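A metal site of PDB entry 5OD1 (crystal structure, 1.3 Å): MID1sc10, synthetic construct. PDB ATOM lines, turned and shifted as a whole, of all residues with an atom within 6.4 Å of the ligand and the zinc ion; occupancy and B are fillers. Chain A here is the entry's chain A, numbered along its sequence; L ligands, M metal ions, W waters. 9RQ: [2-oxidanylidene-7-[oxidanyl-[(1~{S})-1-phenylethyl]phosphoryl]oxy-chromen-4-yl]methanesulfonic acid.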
ATOM      1  N   ARG A  30       7.795  23.907  15.136  1.00  0.00           N
ATOM      2  CA  ARG A  30       6.523  24.238  15.726  1.00  0.00           C
ATOM      3  C   ARG A  30       5.410  23.332  15.196  1.00  0.00           C
ATOM      4  O   ARG A  30       4.596  22.814  15.940  1.00  0.00           O
ATOM      5  CB  ARG A  30       6.188  25.694  15.413  1.00  0.00           C
ATOM      6  CG  ARG A  30       4.886  26.165  16.030  1.00  0.00           C
ATOM      7  CD  ARG A  30       4.562  27.673  15.837  1.00  0.00           C
ATOM      8  NE  ARG A  30       5.371  28.427  14.839  1.00  0.00           N
ATOM      9  CZ  ARG A  30       5.098  28.579  13.544  1.00  0.00           C
ATOM     10  NH1 ARG A  30       4.010  28.053  12.972  1.00  0.00           N
ATOM     11  NH2 ARG A  30       5.938  29.277  12.782  1.00  0.00           N
ATOM     12  N   GLN A  33       5.902  19.831  16.631  1.00  0.00           N
ATOM     13  CA  GLN A  33       5.443  19.792  18.053  1.00  0.00           C
ATOM     14  C   GLN A  33       3.962  19.746  18.158  1.00  0.00           C
ATOM     15  O   GLN A  33       3.426  19.018  18.989  1.00  0.00           O
ATOM     16  CB  GLN A  33       6.005  20.982  18.822  1.00  0.00           C
ATOM     17  CG  GLN A  33       7.500  20.894  19.068  1.00  0.00           C
ATOM     18  CD  GLN A  33       8.100  22.103  19.781  1.00  0.00           C
ATOM     19  OE1 GLN A  33       9.320  22.087  20.170  1.00  0.00           O
ATOM     20  NE2 GLN A  33       7.341  23.117  19.967  1.00  0.00           N
ATOM     21  N   GLN A  34       3.262  20.515  17.337  1.00  0.00           N
ATOM     22  CA  GLN A  34       1.810  20.457  17.310  1.00  0.00           C
ATOM     23  C   GLN A  34       1.259  19.121  16.847  1.00  0.00           C
ATOM     24  O   GLN A  34       0.210  18.689  17.275  1.00  0.00           O
ATOM     25  CB  GLN A  34       1.301  21.637  16.514  1.00  0.00           C
ATOM     26  CG  GLN A  34       1.564  22.956  17.220  1.00  0.00           C
ATOM     27  CD  GLN A  34       1.166  24.125  16.396  1.00  0.00           C
ATOM     28  OE1 GLN A  34       1.794  24.430  15.369  1.00  0.00           O
ATOM     29  NE2 GLN A  34       0.095  24.743  16.788  1.00  0.00           N
ATOM     30  N   ASN A  35       1.950  18.468  15.970  1.00  0.00           N
ATOM     31  CA  ASN A  35       1.594  17.082  15.547  1.00  0.00           C
ATOM     32  C   ASN A  35       1.796  16.078  16.710  1.00  0.00           C
ATOM     33  O   ASN A  35       1.032  15.162  16.880  1.00  0.00           O
ATOM     34  CB  ASN A  35       2.454  16.604  14.376  1.00  0.00           C
ATOM     35  CG  ASN A  35       2.176  17.295  13.041  1.00  0.00           C
ATOM     36  OD1 ASN A  35       3.066  17.291  12.157  1.00  0.00           O
ATOM     37  ND2 ASN A  35       1.003  17.804  12.849  1.00  0.00           N
ATOM     38  N   LEU A  36       2.854  16.288  17.499  1.00  0.00           N
ATOM     39  CA  LEU A  36       3.126  15.424  18.643  1.00  0.00           C
ATOM     40  C   LEU A  36       2.045  15.511  19.715  1.00  0.00           C
ATOM     41  O   LEU A  36       1.706  14.509  20.311  1.00  0.00           O
ATOM     42  CB  LEU A  36       4.482  15.800  19.203  1.00  0.00           C
ATOM     43  CG  LEU A  36       4.974  14.935  20.350  1.00  0.00           C
ATOM     44  CD1 LEU A  36       5.159  13.509  19.931  1.00  0.00           C
ATOM     45  CD2 LEU A  36       6.293  15.521  20.882  1.00  0.00           C
ATOM     46  N   HIS A  37       1.576  16.745  19.941  1.00  0.00           N
ATOM     47  CA  HIS A  37       0.546  17.001  20.959  1.00  0.00           C
ATOM     48  C   HIS A  37      -0.583  15.974  21.095  1.00  0.00           C
ATOM     49  O   HIS A  37      -0.701  15.299  22.114  1.00  0.00           O
ATOM     50  CB  HIS A  37       0.068  18.450  20.842  1.00  0.00           C
ATOM     51  CG  HIS A  37      -1.097  18.764  21.682  1.00  0.00           C
ATOM     52  ND1 HIS A  37      -0.974  19.162  22.987  1.00  0.00           N
ATOM     53  CD2 HIS A  37      -2.424  18.772  21.389  1.00  0.00           C
ATOM     54  CE1 HIS A  37      -2.188  19.351  23.478  1.00  0.00           C
ATOM     55  NE2 HIS A  37      -3.085  19.139  22.529  1.00  0.00           N
ATOM     56  N   PRO A  38      -1.383  15.750  20.011  1.00  0.00           N
ATOM     57  CA  PRO A  38      -2.514  14.834  20.182  1.00  0.00           C
ATOM     58  C   PRO A  38      -2.041  13.365  20.290  1.00  0.00           C
ATOM     59  O   PRO A  38      -2.754  12.545  20.912  1.00  0.00           O
ATOM     60  CB  PRO A  38      -3.354  15.097  18.918  1.00  0.00           C
ATOM     61  CG  PRO A  38      -2.358  15.571  17.888  1.00  0.00           C
ATOM     62  CD  PRO A  38      -1.462  16.462  18.724  1.00  0.00           C
ATOM     63  N   TRP A  40       0.700  12.171  21.718  1.00  0.00           N
ATOM     64  CA  TRP A  40       1.176  11.930  23.130  1.00  0.00           C
ATOM     65  C   TRP A  40      -0.054  11.905  24.023  1.00  0.00           C
ATOM     66  O   TRP A  40      -0.153  11.078  24.918  1.00  0.00           O
ATOM     67  CB  TRP A  40       2.184  12.985  23.533  1.00  0.00           C
ATOM     68  CG  TRP A  40       2.457  12.785  24.990  1.00  0.00           C
ATOM     69  CD1 TRP A  40       1.911  13.490  26.003  1.00  0.00           C
ATOM     70  CD2 TRP A  40       3.194  11.712  25.599  1.00  0.00           C
ATOM     71  NE1 TRP A  40       2.304  12.967  27.213  1.00  0.00           N
ATOM     72  CE2 TRP A  40       3.101  11.873  26.994  1.00  0.00           C
ATOM     73  CE3 TRP A  40       3.926  10.644  25.083  1.00  0.00           C
ATOM     74  CZ2 TRP A  40       3.660  10.974  27.873  1.00  0.00           C
ATOM     75  CZ3 TRP A  40       4.548   9.766  25.972  1.00  0.00           C
ATOM     76  CH2 TRP A  40       4.374   9.936  27.367  1.00  0.00           C
ATOM     77  N   ALA A  41      -0.965  12.874  23.860  1.00  0.00           N
ATOM     78  CA  ALA A  41      -2.124  12.888  24.735  1.00  0.00           C
ATOM     79  C   ALA A  41      -2.881  11.559  24.699  1.00  0.00           C
ATOM     80  O   ALA A  41      -3.347  11.044  25.752  1.00  0.00           O
ATOM     81  CB  ALA A  41      -3.013  14.086  24.464  1.00  0.00           C
ATOM     82  N   ILE A  59       6.870  12.586  31.826  1.00  0.00           N
ATOM     83  CA  ILE A  59       6.719  13.328  30.533  1.00  0.00           C
ATOM     84  C   ILE A  59       5.428  14.160  30.553  1.00  0.00           C
ATOM     85  O   ILE A  59       5.434  15.365  30.200  1.00  0.00           O
ATOM     86  CB  ILE A  59       6.750  12.341  29.368  1.00  0.00           C
ATOM     87  CG1 ILE A  59       8.212  11.796  29.179  1.00  0.00           C
ATOM     88  CG2 ILE A  59       6.370  13.083  28.056  1.00  0.00           C
ATOM     89  CD1 ILE A  59       8.301  10.465  28.445  1.00  0.00           C
ATOM     90  N   GLN A  60       4.326  13.517  30.933  1.00  0.00           N
ATOM     91  CA  GLN A  60       3.041  14.249  30.905  1.00  0.00           C
ATOM     92  C   GLN A  60       3.018  15.423  31.879  1.00  0.00           C
ATOM     93  O   GLN A  60       2.452  16.450  31.612  1.00  0.00           O
ATOM     94  CB  GLN A  60       1.893  13.334  31.166  1.00  0.00           C
ATOM     95  CG  GLN A  60       0.509  13.947  31.229  1.00  0.00           C
ATOM     96  CD  GLN A  60       0.036  14.629  29.936  1.00  0.00           C
ATOM     97  OE1 GLN A  60       0.727  14.664  28.923  1.00  0.00           O
ATOM     98  NE2 GLN A  60      -1.127  15.193  30.025  1.00  0.00           N
ATOM     99  N   GLY A  62       5.500  17.311  32.677  1.00  0.00           N
ATOM    100  CA  GLY A  62       6.210  18.370  31.984  1.00  0.00           C
ATOM    101  C   GLY A  62       5.333  18.965  30.853  1.00  0.00           C
ATOM    102  O   GLY A  62       5.303  20.152  30.658  1.00  0.00           O
ATOM    103  N   HIS A  63       4.647  18.105  30.103  1.00  0.00           N
ATOM    104  CA  HIS A  63       3.751  18.571  29.042  1.00  0.00           C
ATOM    105  C   HIS A  63       2.706  19.571  29.575  1.00  0.00           C
ATOM    106  O   HIS A  63       2.461  20.612  28.941  1.00  0.00           O
ATOM    107  CB  HIS A  63       3.063  17.334  28.437  1.00  0.00           C
ATOM    108  CG  HIS A  63       2.166  17.609  27.275  1.00  0.00           C
ATOM    109  ND1 HIS A  63       1.045  16.867  27.035  1.00  0.00           N
ATOM    110  CD2 HIS A  63       2.235  18.555  26.326  1.00  0.00           C
ATOM    111  CE1 HIS A  63       0.466  17.362  25.943  1.00  0.00           C
ATOM    112  NE2 HIS A  63       1.188  18.365  25.497  1.00  0.00           N
ATOM    113  N   ILE A  66       4.399  22.840  30.376  1.00  0.00           N
ATOM    114  CA  ILE A  66       4.672  23.562  29.142  1.00  0.00           C
ATOM    115  C   ILE A  66       3.439  24.337  28.658  1.00  0.00           C
ATOM    116  O   ILE A  66       3.554  25.532  28.313  1.00  0.00           O
ATOM    117  CB  ILE A  66       5.131  22.565  28.022  1.00  0.00           C
ATOM    118  CG1 ILE A  66       6.550  22.057  28.282  1.00  0.00           C
ATOM    119  CG2 ILE A  66       5.113  23.215  26.621  1.00  0.00           C
ATOM    120  CD1 ILE A  66       6.949  20.796  27.589  1.00  0.00           C
ATOM    121  N   HIS A  67       2.252  23.689  28.662  1.00  0.00           N
ATOM    122  CA  HIS A  67       1.065  24.414  28.198  1.00  0.00           C
ATOM    123  C   HIS A  67       0.774  25.608  29.106  1.00  0.00           C
ATOM    124  O   HIS A  67       0.452  26.702  28.641  1.00  0.00           O
ATOM    125  CB  HIS A  67      -0.142  23.495  28.113  1.00  0.00           C
ATOM    126  CG  HIS A  67      -0.160  22.707  26.858  1.00  0.00           C
ATOM    127  ND1 HIS A  67      -0.849  23.162  25.736  1.00  0.00           N
ATOM    128  CD2 HIS A  67       0.481  21.580  26.487  1.00  0.00           C
ATOM    129  CE1 HIS A  67      -0.624  22.307  24.747  1.00  0.00           C
ATOM    130  NE2 HIS A  67       0.122  21.312  25.188  1.00  0.00           N
ATOM    131  N   ARG A  70       3.428  28.343  28.346  1.00  0.00           N
ATOM    132  CA  ARG A  70       3.276  28.955  27.033  1.00  0.00           C
ATOM    133  C   ARG A  70       2.100  29.936  27.031  1.00  0.00           C
ATOM    134  O   ARG A  70       2.222  31.070  26.579  1.00  0.00           O
ATOM    135  CB  ARG A  70       3.074  27.870  25.967  1.00  0.00           C
ATOM    136  CG  ARG A  70       3.105  28.429  24.551  1.00  0.00           C
ATOM    137  CD  ARG A  70       2.814  27.384  23.488  1.00  0.00           C
ATOM    138  NE  ARG A  70       3.810  26.372  23.397  1.00  0.00           N
ATOM    139  CZ  ARG A  70       3.662  25.066  23.705  1.00  0.00           C
ATOM    140  NH1 ARG A  70       2.519  24.515  24.211  1.00  0.00           N
ATOM    141  NH2 ARG A  70       4.710  24.322  23.558  1.00  0.00           N
ATOM    142  N   ALA A  71       0.979  29.506  27.616  1.00  0.00           N
ATOM    143  CA  ALA A  71      -0.216  30.348  27.603  1.00  0.00           C
ATOM    144  C   ALA A  71       0.004  31.650  28.415  1.00  0.00           C
ATOM    145  O   ALA A  71      -0.525  32.706  28.092  1.00  0.00           O
ATOM    146  CB  ALA A  71      -1.408  29.587  28.128  1.00  0.00           C
ATOM    147  N   SER A  82      10.323  22.539  27.447  1.00  0.00           N
ATOM    148  CA  SER A  82      10.206  21.811  26.178  1.00  0.00           C
ATOM    149  C   SER A  82      11.467  21.006  25.922  1.00  0.00           C
ATOM    150  O   SER A  82      11.405  19.802  25.651  1.00  0.00           O
ATOM    151  CB  SER A  82       9.949  22.755  25.000  1.00  0.00           C
ATOM    152  OG  SER A  82       8.714  23.399  25.163  1.00  0.00           O
ATOM    153  N   THR A  85      11.642  17.990  28.392  1.00  0.00           N
ATOM    154  CA  THR A  85      10.585  17.030  28.246  1.00  0.00           C
ATOM    155  C   THR A  85      10.728  16.280  26.910  1.00  0.00           C
ATOM    156  O   THR A  85      10.544  15.060  26.870  1.00  0.00           O
ATOM    157  CB  THR A  85       9.213  17.705  28.451  1.00  0.00           C
ATOM    158  OG1 THR A  85       9.161  18.323  29.749  1.00  0.00           O
ATOM    159  CG2 THR A  85       8.075  16.684  28.306  1.00  0.00           C
ATOM    160  N   LEU A  86      11.100  16.965  25.851  1.00  0.00           N
ATOM    161  CA  LEU A  86      11.297  16.226  24.588  1.00  0.00           C
ATOM    162  C   LEU A  86      12.480  15.265  24.643  1.00  0.00           C
ATOM    163  O   LEU A  86      12.465  14.147  24.069  1.00  0.00           O
ATOM    164  CB  LEU A  86      11.386  17.159  23.410  1.00  0.00           C
ATOM    165  CG  LEU A  86      10.115  17.926  23.063  1.00  0.00           C
ATOM    166  CD1 LEU A  86      10.420  19.052  22.081  1.00  0.00           C
ATOM    167  CD2 LEU A  86       9.051  16.981  22.540  1.00  0.00           C
ATOM    168  N   MET A  89      11.266  12.222  26.407  1.00  0.00           N
ATOM    169  CA  MET A  89      10.408  11.371  25.537  1.00  0.00           C
ATOM    170  C   MET A  89      11.259  10.585  24.536  1.00  0.00           C
ATOM    171  O   MET A  89      11.002   9.372  24.285  1.00  0.00           O
ATOM    172  CB  MET A  89       9.340  12.253  24.854  1.00  0.00           C
ATOM    173  CG  MET A  89       8.127  11.447  24.369  1.00  0.00           C
ATOM    174  SD  MET A  89       7.091  12.322  23.197  1.00  0.00           S
ATOM    175  CE  MET A  89       6.358  13.589  24.274  1.00  0.00           C
HETATM  176  C4  9RQ L   1       4.020  17.487  23.167  1.00  0.00           C
HETATM  177  C14 9RQ L   1      -0.435  26.579  19.938  1.00  0.00           C
HETATM  178  C5  9RQ L   1       3.940  16.379  23.998  1.00  0.00           C
HETATM  179  C6  9RQ L   1       4.651  16.335  25.170  1.00  0.00           C
HETATM  180  C11 9RQ L   1       0.863  23.989  20.812  1.00  0.00           C
HETATM  181  C7  9RQ L   1       5.432  17.409  25.518  1.00  0.00           C
HETATM  182  C8  9RQ L   1       5.526  18.517  24.691  1.00  0.00           C
HETATM  183  C9  9RQ L   1       2.850  22.689  21.013  1.00  0.00           C
HETATM  184  C10 9RQ L   1       1.474  22.813  21.159  1.00  0.00           C
HETATM  185  C12 9RQ L   1       1.601  25.081  20.332  1.00  0.00           C
HETATM  186  C13 9RQ L   1       1.055  26.356  19.935  1.00  0.00           C
HETATM  187  C3  9RQ L   1       4.759  18.591  23.538  1.00  0.00           C
HETATM  188  O1  9RQ L   1       2.079  19.957  22.924  1.00  0.00           O
HETATM  189  P1  9RQ L   1       3.349  20.783  22.779  1.00  0.00           P
HETATM  190  C1  9RQ L   1       4.851  19.768  22.585  1.00  0.00           C
HETATM  191  C2  9RQ L   1       6.129  20.597  22.677  1.00  0.00           C
HETATM  192  O2  9RQ L   1       3.450  21.482  21.322  1.00  0.00           O
HETATM  193  S1  9RQ L   1      -1.135  27.271  21.429  1.00  0.00           S
HETATM  194  O3  9RQ L   1       0.100  27.870  22.158  1.00  0.00           O
HETATM  195  O4  9RQ L   1      -1.958  28.315  20.893  1.00  0.00           O
HETATM  196  O5  9RQ L   1      -1.746  26.182  22.135  1.00  0.00           O
HETATM  197  C15 9RQ L   1       1.898  27.309  19.479  1.00  0.00           C
HETATM  198  C16 9RQ L   1       3.304  27.125  19.408  1.00  0.00           C
HETATM  199  O6  9RQ L   1       3.809  25.890  19.771  1.00  0.00           O
HETATM  200  O7  9RQ L   1       4.134  27.919  19.054  1.00  0.00           O
HETATM  201  C17 9RQ L   1       2.982  24.887  20.196  1.00  0.00           C
HETATM  202  C18 9RQ L   1       3.619  23.721  20.529  1.00  0.00           C
HETATM  203  O8  9RQ L   1       3.538  21.808  23.865  1.00  0.00           O
HETATM  204 ZN    ZN M   1       0.673  19.705  24.058  1.00  0.00          ZN
HETATM  205  O   HOH W   1       1.227  30.338  22.118  1.00  0.00           O
HETATM  206  O   HOH W   2      -0.427  28.972  24.373  1.00  0.00           O
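An oxygen (O8) of the ligand is in salt-bridge range of the guanidinium group of Arg 70 (2.8 Å).
A ring nitrogen (ND1) of His 63 is in hydrogen-bond range of the side-chain amide oxygen (OE1) of Gln 60, at 2.9 Å. The side-chain amide oxygen of Gln 34 sits close to the backbone carbonyl oxygen of Arg 30 (3.3 Å). NE1 of Trp 40 lies within hydrogen-bond range of OE1 of Gln 60, 2.9 Å away.
The backbone carbonyl oxygen (O) of Gln 33 lies close to an oxygen (O2) of the ligand. Merely in contact with the ligand: Arg 30, Gln 34, Leu 36, Trp 40, Ile 66, Thr 85 and Met 89. Hydrophobic or aromatic side chains that line the ligand: Leu 36, His 37, Trp 40, His 63, Ile 66 and Met 89. Of the 21 residues printed, 12 come within 4 Å of the ligand. The nearest printed residue that does not touch the ligand is Leu 86 (4.4 Å).
Of the 21 residues printed, 3 come within 4 Å of the zinc ion. The nearest printed residue that does not touch the zinc ion is Arg 70 (5.2 Å).
An oxygen (O1) of the ligand binds the zinc ion, 1.8 Å away. The zinc ion is bound by a ring nitrogen (NE2) of His 63. ND1 of His 37 is bound to the zinc ion (2.0 Å). The zinc ion is bound by NE2 of His 67 (2.0 Å).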
